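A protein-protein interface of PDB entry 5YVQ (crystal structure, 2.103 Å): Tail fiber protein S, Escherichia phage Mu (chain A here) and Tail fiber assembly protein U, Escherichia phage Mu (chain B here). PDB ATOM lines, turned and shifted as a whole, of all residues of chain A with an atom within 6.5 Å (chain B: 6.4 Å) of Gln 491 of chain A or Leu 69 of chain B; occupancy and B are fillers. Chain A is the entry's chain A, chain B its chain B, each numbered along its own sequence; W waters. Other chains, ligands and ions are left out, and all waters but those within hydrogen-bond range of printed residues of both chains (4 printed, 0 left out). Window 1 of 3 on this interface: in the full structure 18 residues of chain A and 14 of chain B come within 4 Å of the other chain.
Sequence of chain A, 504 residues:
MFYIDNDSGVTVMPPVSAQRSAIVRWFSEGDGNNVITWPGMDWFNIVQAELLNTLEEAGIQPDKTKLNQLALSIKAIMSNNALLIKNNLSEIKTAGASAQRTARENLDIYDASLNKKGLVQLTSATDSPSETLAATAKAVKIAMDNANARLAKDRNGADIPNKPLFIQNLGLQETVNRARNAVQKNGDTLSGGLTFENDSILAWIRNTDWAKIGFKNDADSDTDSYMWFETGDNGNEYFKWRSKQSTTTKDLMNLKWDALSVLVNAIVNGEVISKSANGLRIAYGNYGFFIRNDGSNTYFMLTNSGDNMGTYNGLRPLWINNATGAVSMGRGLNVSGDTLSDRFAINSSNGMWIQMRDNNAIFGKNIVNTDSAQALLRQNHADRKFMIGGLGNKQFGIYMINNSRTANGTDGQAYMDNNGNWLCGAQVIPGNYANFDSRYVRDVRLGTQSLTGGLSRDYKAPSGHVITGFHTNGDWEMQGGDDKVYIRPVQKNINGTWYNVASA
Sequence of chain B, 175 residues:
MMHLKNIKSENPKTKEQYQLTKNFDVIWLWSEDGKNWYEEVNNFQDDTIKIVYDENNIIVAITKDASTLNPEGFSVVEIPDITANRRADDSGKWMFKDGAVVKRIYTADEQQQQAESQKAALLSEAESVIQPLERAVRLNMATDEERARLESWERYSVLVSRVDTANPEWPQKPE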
ATOM      1  N   VAL A 441      21.509 -12.264  25.786  1.00  0.00           N
ATOM      2  CA  VAL A 441      20.053 -12.263  25.716  1.00  0.00           C
ATOM      3  C   VAL A 441      19.556 -13.637  26.130  1.00  0.00           C
ATOM      4  O   VAL A 441      19.982 -14.655  25.570  1.00  0.00           O
ATOM      5  CB  VAL A 441      19.570 -11.913  24.294  1.00  0.00           C
ATOM      6  CG1 VAL A 441      18.054 -12.020  24.205  1.00  0.00           C
ATOM      7  CG2 VAL A 441      20.023 -10.520  23.899  1.00  0.00           C
ATOM      8  N   ASP A 443      16.028 -14.162  26.375  1.00  0.00           N
ATOM      9  CA  ASP A 443      14.712 -14.351  25.782  1.00  0.00           C
ATOM     10  C   ASP A 443      14.400 -13.136  24.923  1.00  0.00           C
ATOM     11  O   ASP A 443      14.969 -12.057  25.119  1.00  0.00           O
ATOM     12  CB  ASP A 443      13.628 -14.563  26.852  1.00  0.00           C
ATOM     13  CG  ASP A 443      12.408 -15.309  26.314  1.00  0.00           C
ATOM     14  OD1 ASP A 443      12.415 -15.692  25.122  1.00  0.00           O
ATOM     15  OD2 ASP A 443      11.431 -15.496  27.081  1.00  0.00           O
ATOM     16  N   VAL A 444      13.512 -13.339  23.947  1.00  0.00           N
ATOM     17  CA  VAL A 444      12.986 -12.276  23.101  1.00  0.00           C
ATOM     18  C   VAL A 444      11.494 -12.524  22.934  1.00  0.00           C
ATOM     19  O   VAL A 444      11.038 -13.671  22.905  1.00  0.00           O
ATOM     20  CB  VAL A 444      13.684 -12.205  21.717  1.00  0.00           C
ATOM     21  CG1 VAL A 444      15.051 -11.566  21.824  1.00  0.00           C
ATOM     22  CG2 VAL A 444      13.825 -13.587  21.111  1.00  0.00           C
ATOM     23  N   ARG A 445      10.726 -11.442  22.827  1.00  0.00           N
ATOM     24  CA  ARG A 445       9.278 -11.545  22.726  1.00  0.00           C
ATOM     25  C   ARG A 445       8.726 -10.264  22.115  1.00  0.00           C
ATOM     26  O   ARG A 445       9.428  -9.256  21.987  1.00  0.00           O
ATOM     27  CB  ARG A 445       8.645 -11.801  24.094  1.00  0.00           C
ATOM     28  CG  ARG A 445       8.517 -10.545  24.932  1.00  0.00           C
ATOM     29  CD  ARG A 445       7.888 -10.834  26.276  1.00  0.00           C
ATOM     30  NE  ARG A 445       7.836  -9.633  27.096  1.00  0.00           N
ATOM     31  CZ  ARG A 445       7.554  -9.629  28.394  1.00  0.00           C
ATOM     32  NH1 ARG A 445       7.281 -10.767  29.020  1.00  0.00           N
ATOM     33  NH2 ARG A 445       7.539  -8.481  29.064  1.00  0.00           N
ATOM     34  N   LEU A 446       7.451 -10.329  21.727  1.00  0.00           N
ATOM     35  CA  LEU A 446       6.683  -9.155  21.340  1.00  0.00           C
ATOM     36  C   LEU A 446       5.798  -8.737  22.512  1.00  0.00           C
ATOM     37  O   LEU A 446       5.071  -9.563  23.071  1.00  0.00           O
ATOM     38  CB  LEU A 446       5.830  -9.443  20.101  1.00  0.00           C
ATOM     39  CG  LEU A 446       6.590 -10.025  18.903  1.00  0.00           C
ATOM     40  CD1 LEU A 446       5.624 -10.526  17.844  1.00  0.00           C
ATOM     41  CD2 LEU A 446       7.589  -9.022  18.318  1.00  0.00           C
ATOM     42  N   GLY A 447       5.873  -7.462  22.889  1.00  0.00           N
ATOM     43  CA  GLY A 447       5.082  -6.937  23.982  1.00  0.00           C
ATOM     44  C   GLY A 447       3.641  -6.624  23.588  1.00  0.00           C
ATOM     45  O   GLY A 447       3.157  -6.970  22.508  1.00  0.00           O
ATOM     46  N   THR A 448       2.958  -5.931  24.496  1.00  0.00           N
ATOM     47  CA  THR A 448       1.520  -5.721  24.378  1.00  0.00           C
ATOM     48  C   THR A 448       1.168  -4.891  23.148  1.00  0.00           C
ATOM     49  O   THR A 448       1.838  -3.907  22.820  1.00  0.00           O
ATOM     50  CB  THR A 448       0.982  -5.043  25.641  1.00  0.00           C
ATOM     51  OG1 THR A 448       0.887  -6.012  26.692  1.00  0.00           O
ATOM     52  CG2 THR A 448      -0.405  -4.403  25.396  1.00  0.00           C
ATOM     53  N   GLY A 464      11.461   0.840  18.570  1.00  0.00           N
ATOM     54  CA  GLY A 464      11.357  -0.519  19.050  1.00  0.00           C
ATOM     55  C   GLY A 464      10.138  -1.290  18.593  1.00  0.00           C
ATOM     56  O   GLY A 464      10.058  -2.494  18.874  1.00  0.00           O
ATOM     57  N   PRO A 489       5.715  -3.713  20.691  1.00  0.00           N
ATOM     58  CA  PRO A 489       7.148  -3.506  20.925  1.00  0.00           C
ATOM     59  C   PRO A 489       7.916  -4.817  20.972  1.00  0.00           C
ATOM     60  O   PRO A 489       7.498  -5.797  21.596  1.00  0.00           O
ATOM     61  CB  PRO A 489       7.170  -2.814  22.295  1.00  0.00           C
ATOM     62  CG  PRO A 489       5.989  -3.411  23.010  1.00  0.00           C
ATOM     63  CD  PRO A 489       4.937  -3.697  21.945  1.00  0.00           C
ATOM     64  N   VAL A 490       9.067  -4.830  20.304  1.00  0.00           N
ATOM     65  CA  VAL A 490       9.988  -5.958  20.424  1.00  0.00           C
ATOM     66  C   VAL A 490      10.763  -5.821  21.730  1.00  0.00           C
ATOM     67  O   VAL A 490      11.269  -4.739  22.057  1.00  0.00           O
ATOM     68  CB  VAL A 490      10.937  -6.029  19.216  1.00  0.00           C
ATOM     69  CG1 VAL A 490      11.907  -7.187  19.388  1.00  0.00           C
ATOM     70  CG2 VAL A 490      10.145  -6.173  17.912  1.00  0.00           C
ATOM     71  N   GLN A 491      10.865  -6.913  22.481  1.00  0.00           N
ATOM     72  CA  GLN A 491      11.485  -6.874  23.799  1.00  0.00           C
ATOM     73  C   GLN A 491      12.536  -7.966  23.941  1.00  0.00           C
ATOM     74  O   GLN A 491      12.407  -9.053  23.373  1.00  0.00           O
ATOM     75  CB  GLN A 491      10.438  -7.017  24.900  1.00  0.00           C
ATOM     76  CG  GLN A 491       9.447  -5.889  24.923  1.00  0.00           C
ATOM     77  CD  GLN A 491       8.561  -5.931  26.138  1.00  0.00           C
ATOM     78  OE1 GLN A 491       8.117  -6.999  26.560  1.00  0.00           O
ATOM     79  NE2 GLN A 491       8.301  -4.766  26.720  1.00  0.00           N
ATOM     80  N   LYS A 492      13.575  -7.663  24.724  1.00  0.00           N
ATOM     81  CA  LYS A 492      14.668  -8.587  25.003  1.00  0.00           C
ATOM     82  C   LYS A 492      14.849  -8.730  26.506  1.00  0.00           C
ATOM     83  O   LYS A 492      14.757  -7.752  27.256  1.00  0.00           O
ATOM     84  CB  LYS A 492      15.991  -8.117  24.377  1.00  0.00           C
ATOM     85  CG  LYS A 492      16.450  -6.761  24.867  1.00  0.00           C
ATOM     86  CD  LYS A 492      17.604  -6.225  24.047  1.00  0.00           C
ATOM     87  CE  LYS A 492      17.920  -4.795  24.436  1.00  0.00           C
ATOM     88  NZ  LYS A 492      18.969  -4.220  23.551  1.00  0.00           N
ATOM     89  N   ASN A 493      15.096  -9.949  26.945  1.00  0.00           N
ATOM     90  CA  ASN A 493      15.303 -10.225  28.358  1.00  0.00           C
ATOM     91  C   ASN A 493      16.803 -10.381  28.599  1.00  0.00           C
ATOM     92  O   ASN A 493      17.412 -11.358  28.154  1.00  0.00           O
ATOM     93  CB  ASN A 493      14.530 -11.469  28.782  1.00  0.00           C
ATOM     94  CG  ASN A 493      14.587 -11.707  30.277  1.00  0.00           C
ATOM     95  OD1 ASN A 493      15.634 -11.565  30.897  1.00  0.00           O
ATOM     96  ND2 ASN A 493      13.462 -12.070  30.862  1.00  0.00           N
ATOM     97  N   TRP A 498      13.066  -7.554  31.322  1.00  0.00           N
ATOM     98  CA  TRP A 498      12.589  -7.300  29.966  1.00  0.00           C
ATOM     99  C   TRP A 498      12.831  -5.838  29.613  1.00  0.00           C
ATOM    100  O   TRP A 498      12.310  -4.941  30.281  1.00  0.00           O
ATOM    101  CB  TRP A 498      11.104  -7.632  29.852  1.00  0.00           C
ATOM    102  CG  TRP A 498      10.843  -9.087  29.707  1.00  0.00           C
ATOM    103  CD1 TRP A 498      10.310  -9.924  30.649  1.00  0.00           C
ATOM    104  CD2 TRP A 498      11.108  -9.892  28.555  1.00  0.00           C
ATOM    105  NE1 TRP A 498      10.236 -11.202  30.153  1.00  0.00           N
ATOM    106  CE2 TRP A 498      10.719 -11.212  28.870  1.00  0.00           C
ATOM    107  CE3 TRP A 498      11.642  -9.627  27.287  1.00  0.00           C
ATOM    108  CZ2 TRP A 498      10.836 -12.261  27.959  1.00  0.00           C
ATOM    109  CZ3 TRP A 498      11.763 -10.670  26.386  1.00  0.00           C
ATOM    110  CH2 TRP A 498      11.359 -11.972  26.726  1.00  0.00           C
ATOM    111  N   TYR A 499      13.629  -5.597  28.576  1.00  0.00           N
ATOM    112  CA  TYR A 499      13.889  -4.249  28.101  1.00  0.00           C
ATOM    113  C   TYR A 499      13.311  -4.091  26.701  1.00  0.00           C
ATOM    114  O   TYR A 499      13.228  -5.050  25.926  1.00  0.00           O
ATOM    115  CB  TYR A 499      15.393  -3.923  28.073  1.00  0.00           C
ATOM    116  CG  TYR A 499      16.088  -3.947  29.422  1.00  0.00           C
ATOM    117  CD1 TYR A 499      16.002  -2.870  30.299  1.00  0.00           C
ATOM    118  CD2 TYR A 499      16.849  -5.046  29.809  1.00  0.00           C
ATOM    119  CE1 TYR A 499      16.643  -2.897  31.535  1.00  0.00           C
ATOM    120  CE2 TYR A 499      17.499  -5.083  31.032  1.00  0.00           C
ATOM    121  CZ  TYR A 499      17.394  -4.008  31.894  1.00  0.00           C
ATOM    122  OH  TYR A 499      18.040  -4.053  33.116  1.00  0.00           O
ATOM    123  N   ASN A 500      12.920  -2.870  26.370  1.00  0.00           N
ATOM    124  CA  ASN A 500      12.425  -2.616  25.031  1.00  0.00           C
ATOM    125  C   ASN A 500      13.586  -2.437  24.061  1.00  0.00           C
ATOM    126  O   ASN A 500      14.591  -1.790  24.370  1.00  0.00           O
ATOM    127  CB  ASN A 500      11.504  -1.400  25.031  1.00  0.00           C
ATOM    128  CG  ASN A 500      10.204  -1.679  25.753  1.00  0.00           C
ATOM    129  OD1 ASN A 500       9.357  -2.414  25.250  1.00  0.00           O
ATOM    130  ND2 ASN A 500      10.054  -1.124  26.953  1.00  0.00           N
ATOM    131  N   VAL A 501      13.448  -3.053  22.892  1.00  0.00           N
ATOM    132  CA  VAL A 501      14.453  -2.944  21.849  1.00  0.00           C
ATOM    133  C   VAL A 501      14.489  -1.515  21.314  1.00  0.00           C
ATOM    134  O   VAL A 501      13.493  -0.786  21.364  1.00  0.00           O
ATOM    135  CB  VAL A 501      14.133  -3.981  20.756  1.00  0.00           C
ATOM    136  CG1 VAL A 501      14.655  -3.568  19.387  1.00  0.00           C
ATOM    137  CG2 VAL A 501      14.677  -5.344  21.181  1.00  0.00           C
ATOM    138  N   LEU B  29      13.546   4.835  30.613  1.00  0.00           N
ATOM    139  CA  LEU B  29      12.306   5.592  30.612  1.00  0.00           C
ATOM    140  C   LEU B  29      12.012   6.120  32.011  1.00  0.00           C
ATOM    141  O   LEU B  29      12.186   5.411  33.006  1.00  0.00           O
ATOM    142  CB  LEU B  29      11.148   4.721  30.122  1.00  0.00           C
ATOM    143  CG  LEU B  29      11.297   4.147  28.708  1.00  0.00           C
ATOM    144  CD1 LEU B  29      10.160   3.182  28.388  1.00  0.00           C
ATOM    145  CD2 LEU B  29      11.374   5.266  27.664  1.00  0.00           C
ATOM    146  N   TRP B  37      10.925   3.695  34.923  1.00  0.00           N
ATOM    147  CA  TRP B  37       9.893   2.740  34.534  1.00  0.00           C
ATOM    148  C   TRP B  37      10.330   1.295  34.775  1.00  0.00           C
ATOM    149  O   TRP B  37       9.546   0.485  35.285  1.00  0.00           O
ATOM    150  CB  TRP B  37       9.526   2.956  33.067  1.00  0.00           C
ATOM    151  CG  TRP B  37       8.868   1.777  32.437  1.00  0.00           C
ATOM    152  CD1 TRP B  37       9.442   0.877  31.585  1.00  0.00           C
ATOM    153  CD2 TRP B  37       7.506   1.365  32.601  1.00  0.00           C
ATOM    154  NE1 TRP B  37       8.519  -0.071  31.211  1.00  0.00           N
ATOM    155  CE2 TRP B  37       7.324   0.205  31.822  1.00  0.00           C
ATOM    156  CE3 TRP B  37       6.421   1.864  33.329  1.00  0.00           C
ATOM    157  CZ2 TRP B  37       6.103  -0.465  31.753  1.00  0.00           C
ATOM    158  CZ3 TRP B  37       5.213   1.195  33.262  1.00  0.00           C
ATOM    159  CH2 TRP B  37       5.066   0.041  32.481  1.00  0.00           C
ATOM    160  N   TYR B  38      11.577   0.953  34.422  1.00  0.00           N
ATOM    161  CA  TYR B  38      11.990  -0.451  34.446  1.00  0.00           C
ATOM    162  C   TYR B  38      12.141  -0.987  35.863  1.00  0.00           C
ATOM    163  O   TYR B  38      11.945  -2.186  36.088  1.00  0.00           O
ATOM    164  CB  TYR B  38      13.295  -0.645  33.665  1.00  0.00           C
ATOM    165  CG  TYR B  38      13.078  -0.647  32.171  1.00  0.00           C
ATOM    166  CD1 TYR B  38      12.252  -1.587  31.572  1.00  0.00           C
ATOM    167  CD2 TYR B  38      13.665   0.322  31.361  1.00  0.00           C
ATOM    168  CE1 TYR B  38      12.036  -1.579  30.207  1.00  0.00           C
ATOM    169  CE2 TYR B  38      13.454   0.337  29.997  1.00  0.00           C
ATOM    170  CZ  TYR B  38      12.644  -0.617  29.426  1.00  0.00           C
ATOM    171  OH  TYR B  38      12.427  -0.595  28.069  1.00  0.00           O
ATOM    172  N   PHE B  44       4.197  -3.209  40.495  1.00  0.00           N
ATOM    173  CA  PHE B  44       2.830  -3.436  40.048  1.00  0.00           C
ATOM    174  C   PHE B  44       2.285  -4.720  40.662  1.00  0.00           C
ATOM    175  O   PHE B  44       3.023  -5.681  40.900  1.00  0.00           O
ATOM    176  CB  PHE B  44       2.762  -3.538  38.521  1.00  0.00           C
ATOM    177  CG  PHE B  44       2.820  -2.216  37.807  1.00  0.00           C
ATOM    178  CD1 PHE B  44       4.039  -1.624  37.513  1.00  0.00           C
ATOM    179  CD2 PHE B  44       1.655  -1.582  37.400  1.00  0.00           C
ATOM    180  CE1 PHE B  44       4.103  -0.418  36.849  1.00  0.00           C
ATOM    181  CE2 PHE B  44       1.705  -0.369  36.730  1.00  0.00           C
ATOM    182  CZ  PHE B  44       2.934   0.215  36.452  1.00  0.00           C
ATOM    183  N   LYS B  50      -3.543  -2.938  33.829  1.00  0.00           N
ATOM    184  CA  LYS B  50      -2.617  -1.834  33.616  1.00  0.00           C
ATOM    185  C   LYS B  50      -3.015  -1.124  32.331  1.00  0.00           C
ATOM    186  O   LYS B  50      -3.108  -1.756  31.271  1.00  0.00           O
ATOM    187  CB  LYS B  50      -1.171  -2.329  33.543  1.00  0.00           C
ATOM    188  CG  LYS B  50      -0.643  -2.915  34.854  1.00  0.00           C
ATOM    189  CD  LYS B  50      -0.939  -4.407  34.954  1.00  0.00           C
ATOM    190  CE  LYS B  50      -0.394  -5.007  36.247  1.00  0.00           C
ATOM    191  NZ  LYS B  50      -1.045  -6.314  36.577  1.00  0.00           N
ATOM    192  N   ILE B  51      -3.251   0.182  32.430  1.00  0.00           N
ATOM    193  CA  ILE B  51      -3.814   0.976  31.346  1.00  0.00           C
ATOM    194  C   ILE B  51      -2.733   1.891  30.791  1.00  0.00           C
ATOM    195  O   ILE B  51      -1.900   2.414  31.543  1.00  0.00           O
ATOM    196  CB  ILE B  51      -5.031   1.789  31.831  1.00  0.00           C
ATOM    197  CG1 ILE B  51      -6.138   0.849  32.311  1.00  0.00           C
ATOM    198  CG2 ILE B  51      -5.543   2.725  30.740  1.00  0.00           C
ATOM    199  CD1 ILE B  51      -7.055   0.357  31.209  1.00  0.00           C
ATOM    200  N   VAL B  52      -2.741   2.071  29.472  1.00  0.00           N
ATOM    201  CA  VAL B  52      -1.855   3.000  28.780  1.00  0.00           C
ATOM    202  C   VAL B  52      -2.723   3.980  28.008  1.00  0.00           C
ATOM    203  O   VAL B  52      -3.490   3.570  27.127  1.00  0.00           O
ATOM    204  CB  VAL B  52      -0.884   2.272  27.839  1.00  0.00           C
ATOM    205  CG1 VAL B  52      -0.178   3.276  26.943  1.00  0.00           C
ATOM    206  CG2 VAL B  52       0.126   1.423  28.655  1.00  0.00           C
ATOM    207  N   ALA B  61      -3.545   1.036  25.032  1.00  0.00           N
ATOM    208  CA  ALA B  61      -3.012  -0.288  25.313  1.00  0.00           C
ATOM    209  C   ALA B  61      -3.465  -0.739  26.694  1.00  0.00           C
ATOM    210  O   ALA B  61      -3.527   0.065  27.629  1.00  0.00           O
ATOM    211  CB  ALA B  61      -1.483  -0.308  25.224  1.00  0.00           C
ATOM    212  N   ILE B  62      -3.780  -2.029  26.809  1.00  0.00           N
ATOM    213  CA  ILE B  62      -4.211  -2.633  28.063  1.00  0.00           C
ATOM    214  C   ILE B  62      -3.481  -3.958  28.233  1.00  0.00           C
ATOM    215  O   ILE B  62      -3.259  -4.687  27.259  1.00  0.00           O
ATOM    216  CB  ILE B  62      -5.741  -2.840  28.106  1.00  0.00           C
ATOM    217  CG1 ILE B  62      -6.471  -1.512  27.897  1.00  0.00           C
ATOM    218  CG2 ILE B  62      -6.173  -3.458  29.428  1.00  0.00           C
ATOM    219  CD1 ILE B  62      -7.815  -1.661  27.235  1.00  0.00           C
ATOM    220  N   THR B  63      -3.106  -4.267  29.471  1.00  0.00           N
ATOM    221  CA  THR B  63      -2.436  -5.523  29.766  1.00  0.00           C
ATOM    222  C   THR B  63      -2.629  -5.841  31.241  1.00  0.00           C
ATOM    223  O   THR B  63      -3.096  -5.011  32.022  1.00  0.00           O
ATOM    224  CB  THR B  63      -0.941  -5.461  29.420  1.00  0.00           C
ATOM    225  OG1 THR B  63      -0.416  -6.788  29.349  1.00  0.00           O
ATOM    226  CG2 THR B  63      -0.167  -4.678  30.484  1.00  0.00           C
ATOM    227  N   ASP B  65       0.275  -7.428  32.480  1.00  0.00           N
ATOM    228  CA  ASP B  65       1.708  -7.607  32.725  1.00  0.00           C
ATOM    229  C   ASP B  65       2.433  -6.350  32.254  1.00  0.00           C
ATOM    230  O   ASP B  65       2.683  -6.180  31.055  1.00  0.00           O
ATOM    231  CB  ASP B  65       2.230  -8.848  32.013  1.00  0.00           C
ATOM    232  CG  ASP B  65       3.724  -9.047  32.196  1.00  0.00           C
ATOM    233  OD1 ASP B  65       4.366  -8.271  32.933  1.00  0.00           O
ATOM    234  OD2 ASP B  65       4.263  -9.998  31.595  1.00  0.00           O
ATOM    235  N   ALA B  66       2.801  -5.492  33.210  1.00  0.00           N
ATOM    236  CA  ALA B  66       3.351  -4.183  32.874  1.00  0.00           C
ATOM    237  C   ALA B  66       4.676  -4.284  32.126  1.00  0.00           C
ATOM    238  O   ALA B  66       5.004  -3.394  31.334  1.00  0.00           O
ATOM    239  CB  ALA B  66       3.521  -3.348  34.143  1.00  0.00           C
ATOM    240  N   SER B  67       5.447  -5.352  32.355  1.00  0.00           N
ATOM    241  CA  SER B  67       6.729  -5.501  31.674  1.00  0.00           C
ATOM    242  C   SER B  67       6.575  -5.684  30.169  1.00  0.00           C
ATOM    243  O   SER B  67       7.559  -5.540  29.435  1.00  0.00           O
ATOM    244  CB  SER B  67       7.517  -6.683  32.261  1.00  0.00           C
ATOM    245  OG  SER B  67       6.904  -7.924  31.945  1.00  0.00           O
ATOM    246  N   THR B  68       5.375  -6.013  29.695  1.00  0.00           N
ATOM    247  CA  THR B  68       5.125  -6.106  28.263  1.00  0.00           C
ATOM    248  C   THR B  68       4.819  -4.755  27.632  1.00  0.00           C
ATOM    249  O   THR B  68       4.520  -4.703  26.433  1.00  0.00           O
ATOM    250  CB  THR B  68       3.975  -7.087  27.985  1.00  0.00           C
ATOM    251  OG1 THR B  68       2.720  -6.483  28.323  1.00  0.00           O
ATOM    252  CG2 THR B  68       4.158  -8.372  28.803  1.00  0.00           C
ATOM    253  N   LEU B  69       4.894  -3.669  28.395  1.00  0.00           N
ATOM    254  CA  LEU B  69       4.590  -2.341  27.892  1.00  0.00           C
ATOM    255  C   LEU B  69       5.865  -1.602  27.497  1.00  0.00           C
ATOM    256  O   LEU B  69       6.945  -1.847  28.038  1.00  0.00           O
ATOM    257  CB  LEU B  69       3.818  -1.528  28.936  1.00  0.00           C
ATOM    258  CG  LEU B  69       2.455  -2.091  29.350  1.00  0.00           C
ATOM    259  CD1 LEU B  69       1.874  -1.309  30.531  1.00  0.00           C
ATOM    260  CD2 LEU B  69       1.487  -2.086  28.170  1.00  0.00           C
ATOM    261  N   ASN B  70       5.725  -0.701  26.521  1.00  0.00           N
ATOM    262  CA  ASN B  70       6.746   0.287  26.170  1.00  0.00           C
ATOM    263  C   ASN B  70       6.067   1.648  26.278  1.00  0.00           C
ATOM    264  O   ASN B  70       5.518   2.162  25.290  1.00  0.00           O
ATOM    265  CB  ASN B  70       7.315   0.052  24.769  1.00  0.00           C
ATOM    266  CG  ASN B  70       8.530   0.923  24.474  1.00  0.00           C
ATOM    267  OD1 ASN B  70       8.831   1.865  25.214  1.00  0.00           O
ATOM    268  ND2 ASN B  70       9.230   0.614  23.386  1.00  0.00           N
ATOM    269  N   PRO B  71       6.065   2.261  27.463  1.00  0.00           N
ATOM    270  CA  PRO B  71       5.254   3.471  27.664  1.00  0.00           C
ATOM    271  C   PRO B  71       5.963   4.769  27.305  1.00  0.00           C
ATOM    272  O   PRO B  71       5.641   5.821  27.866  1.00  0.00           O
ATOM    273  CB  PRO B  71       4.935   3.415  29.161  1.00  0.00           C
ATOM    274  CG  PRO B  71       6.136   2.736  29.756  1.00  0.00           C
ATOM    275  CD  PRO B  71       6.631   1.749  28.726  1.00  0.00           C
ATOM    276  N   VAL B  76       0.919   5.383  32.289  1.00  0.00           N
ATOM    277  CA  VAL B  76       0.498   4.067  32.756  1.00  0.00           C
ATOM    278  C   VAL B  76      -0.189   4.229  34.103  1.00  0.00           C
ATOM    279  O   VAL B  76       0.348   4.885  35.004  1.00  0.00           O
ATOM    280  CB  VAL B  76       1.685   3.089  32.866  1.00  0.00           C
ATOM    281  CG1 VAL B  76       1.221   1.750  33.424  1.00  0.00           C
ATOM    282  CG2 VAL B  76       2.350   2.896  31.520  1.00  0.00           C
HETATM  283  O   HOH W   1       6.786 -11.159  31.829  1.00  0.00           O
HETATM  284  O   HOH W   2      -1.018  -7.736  27.113  1.00  0.00           O
HETATM  285  O   HOH W   3       3.070  -2.101  24.698  1.00  0.00           O
HETATM  286  O   HOH W   4      15.295  -0.110  26.407  1.00  0.00           O
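NH2 of Arg 445 of chain A sits at hydrogen-bond distance from O of Ser 67 of chain B (3.0 Å).
The side-chain hydroxyl (OG1) of Thr 63 of chain B sits at hydrogen-bond distance from the side-chain hydroxyl (OG1) of Thr 448 of chain A (3.1 Å).
OG1 of Thr 68 of chain B sits at hydrogen-bond distance from OG1 of Thr 448 of chain A (2.5 Å).
The side-chain amide nitrogen (NE2) of Gln 491 of chain A sits at hydrogen-bond distance from the backbone carbonyl oxygen (O) of Ser 67 of chain B (2.9 Å).
The side-chain amide nitrogen of Gln 491 of chain A is in hydrogen-bond range of the backbone carbonyl oxygen of Leu 69 of chain B (3.5 Å).
The side-chain hydroxyl of Tyr 38 of chain B is in hydrogen-bond range of the side-chain amide nitrogen of Asn 500 of chain A, 2.7 Å away.
The side-chain amide nitrogen (ND2) of Asn 500 of chain A is in hydrogen-bond range of the backbone carbonyl oxygen (O) of Leu 69 of chain B (3.4 Å).
The guanidinium group of Arg 445 of chain A sits close to the backbone NH of Thr 68 of chain B (3.3 Å).
The backbone NH (N) of Gly 447 of chain A sits at hydrogen-bond distance from the backbone carbonyl oxygen (O) of Pro 489 of chain A, 2.7 Å away.
The side-chain amide nitrogen (NE2) of Gln 491 of chain A lies within hydrogen-bond range of the side-chain amide oxygen (OD1) of Asn 500 of chain A (3.0 Å).
ND2 of Asn 493 of chain A sits close to NE1 of Trp 498 of chain A (3.4 Å).
Thr 68 of chain B touches Gly 447 of chain A (O to CA, 3.4 Å).
Thr 448 of chain A touches Ile 62 of chain B.
Leu 69 of chain B touches Thr 448 of chain A.
Thr 68 of chain B touches Pro 489 of chain A (O to CG, 3.9 Å).
CB of Pro 489 of chain A touches CB of Asn 70 of chain B (3.8 Å).
Tyr 38 of chain B touches Trp 498 of chain A (CE1 to O, 3.4 Å).
OD1 of Asn 500 of chain A touches CB of Asn 70 of chain B, 3.2 Å away.
Printed residues of chain B within 4 Å of Arg 445 of chain A: Ser 67 (3.0 Å) and Thr 68 (3.3 Å).
Of the printed residues of chain B, Thr 448 of chain A touches Ile 62 (3.4 Å), Thr 63 (3.1 Å), Thr 68 (2.5 Å) and Leu 69 (3.9 Å).
Printed residues of chain B within 4 Å of Pro 489 of chain A: Thr 68 (3.9 Å) and Asn 70 (3.8 Å).
Gln 491 of chain A touches just these residues of chain B: Ser 67 (2.9 Å), Thr 68 (3.6 Å) and Leu 69 (3.5 Å).
Ala 61 of chain B touches none of the printed residues of chain A.
Of chain A, only Thr 448 (3.9 Å), Gln 491 (3.5 Å) and Asn 500 (3.4 Å) come within 4 Å of Leu 69 of chain B.
The nearest residue of chain B that does not touch Gln 491 of chain A is Asn 70 of chain B (4.8 Å).
The nearest residue of chain A that does not touch Leu 69 of chain B is Pro 489 of chain A (4.8 Å).
The nearest printed residue of chain A that does not touch Tyr 38 of chain B is Val 501 of chain A (5.8 Å).
Hydrophobic or aromatic side chains of chain B that line the printed part of chain A: Tyr 38 and Leu 69.
Along chain B the printed residues that touch a printed residue of chain A span positions 38 to 70.
Hydrophobic or aromatic side chains of chain A within 4 Å of the printed part of chain B: Pro 489.
Water W2 lies within hydrogen-bond range of OG1 of Thr 63 of chain B (2.5 Å) and OG1 of Thr 448 of chain A (2.6 Å).
Water W1 lies within hydrogen-bond range of OD2 of Asp 65 of chain B, NH1 of Arg 445 of chain A and OG of Ser 67 of chain B.
Water W3 bridges O of Thr 448 of chain A and O of Thr 68 of chain B.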
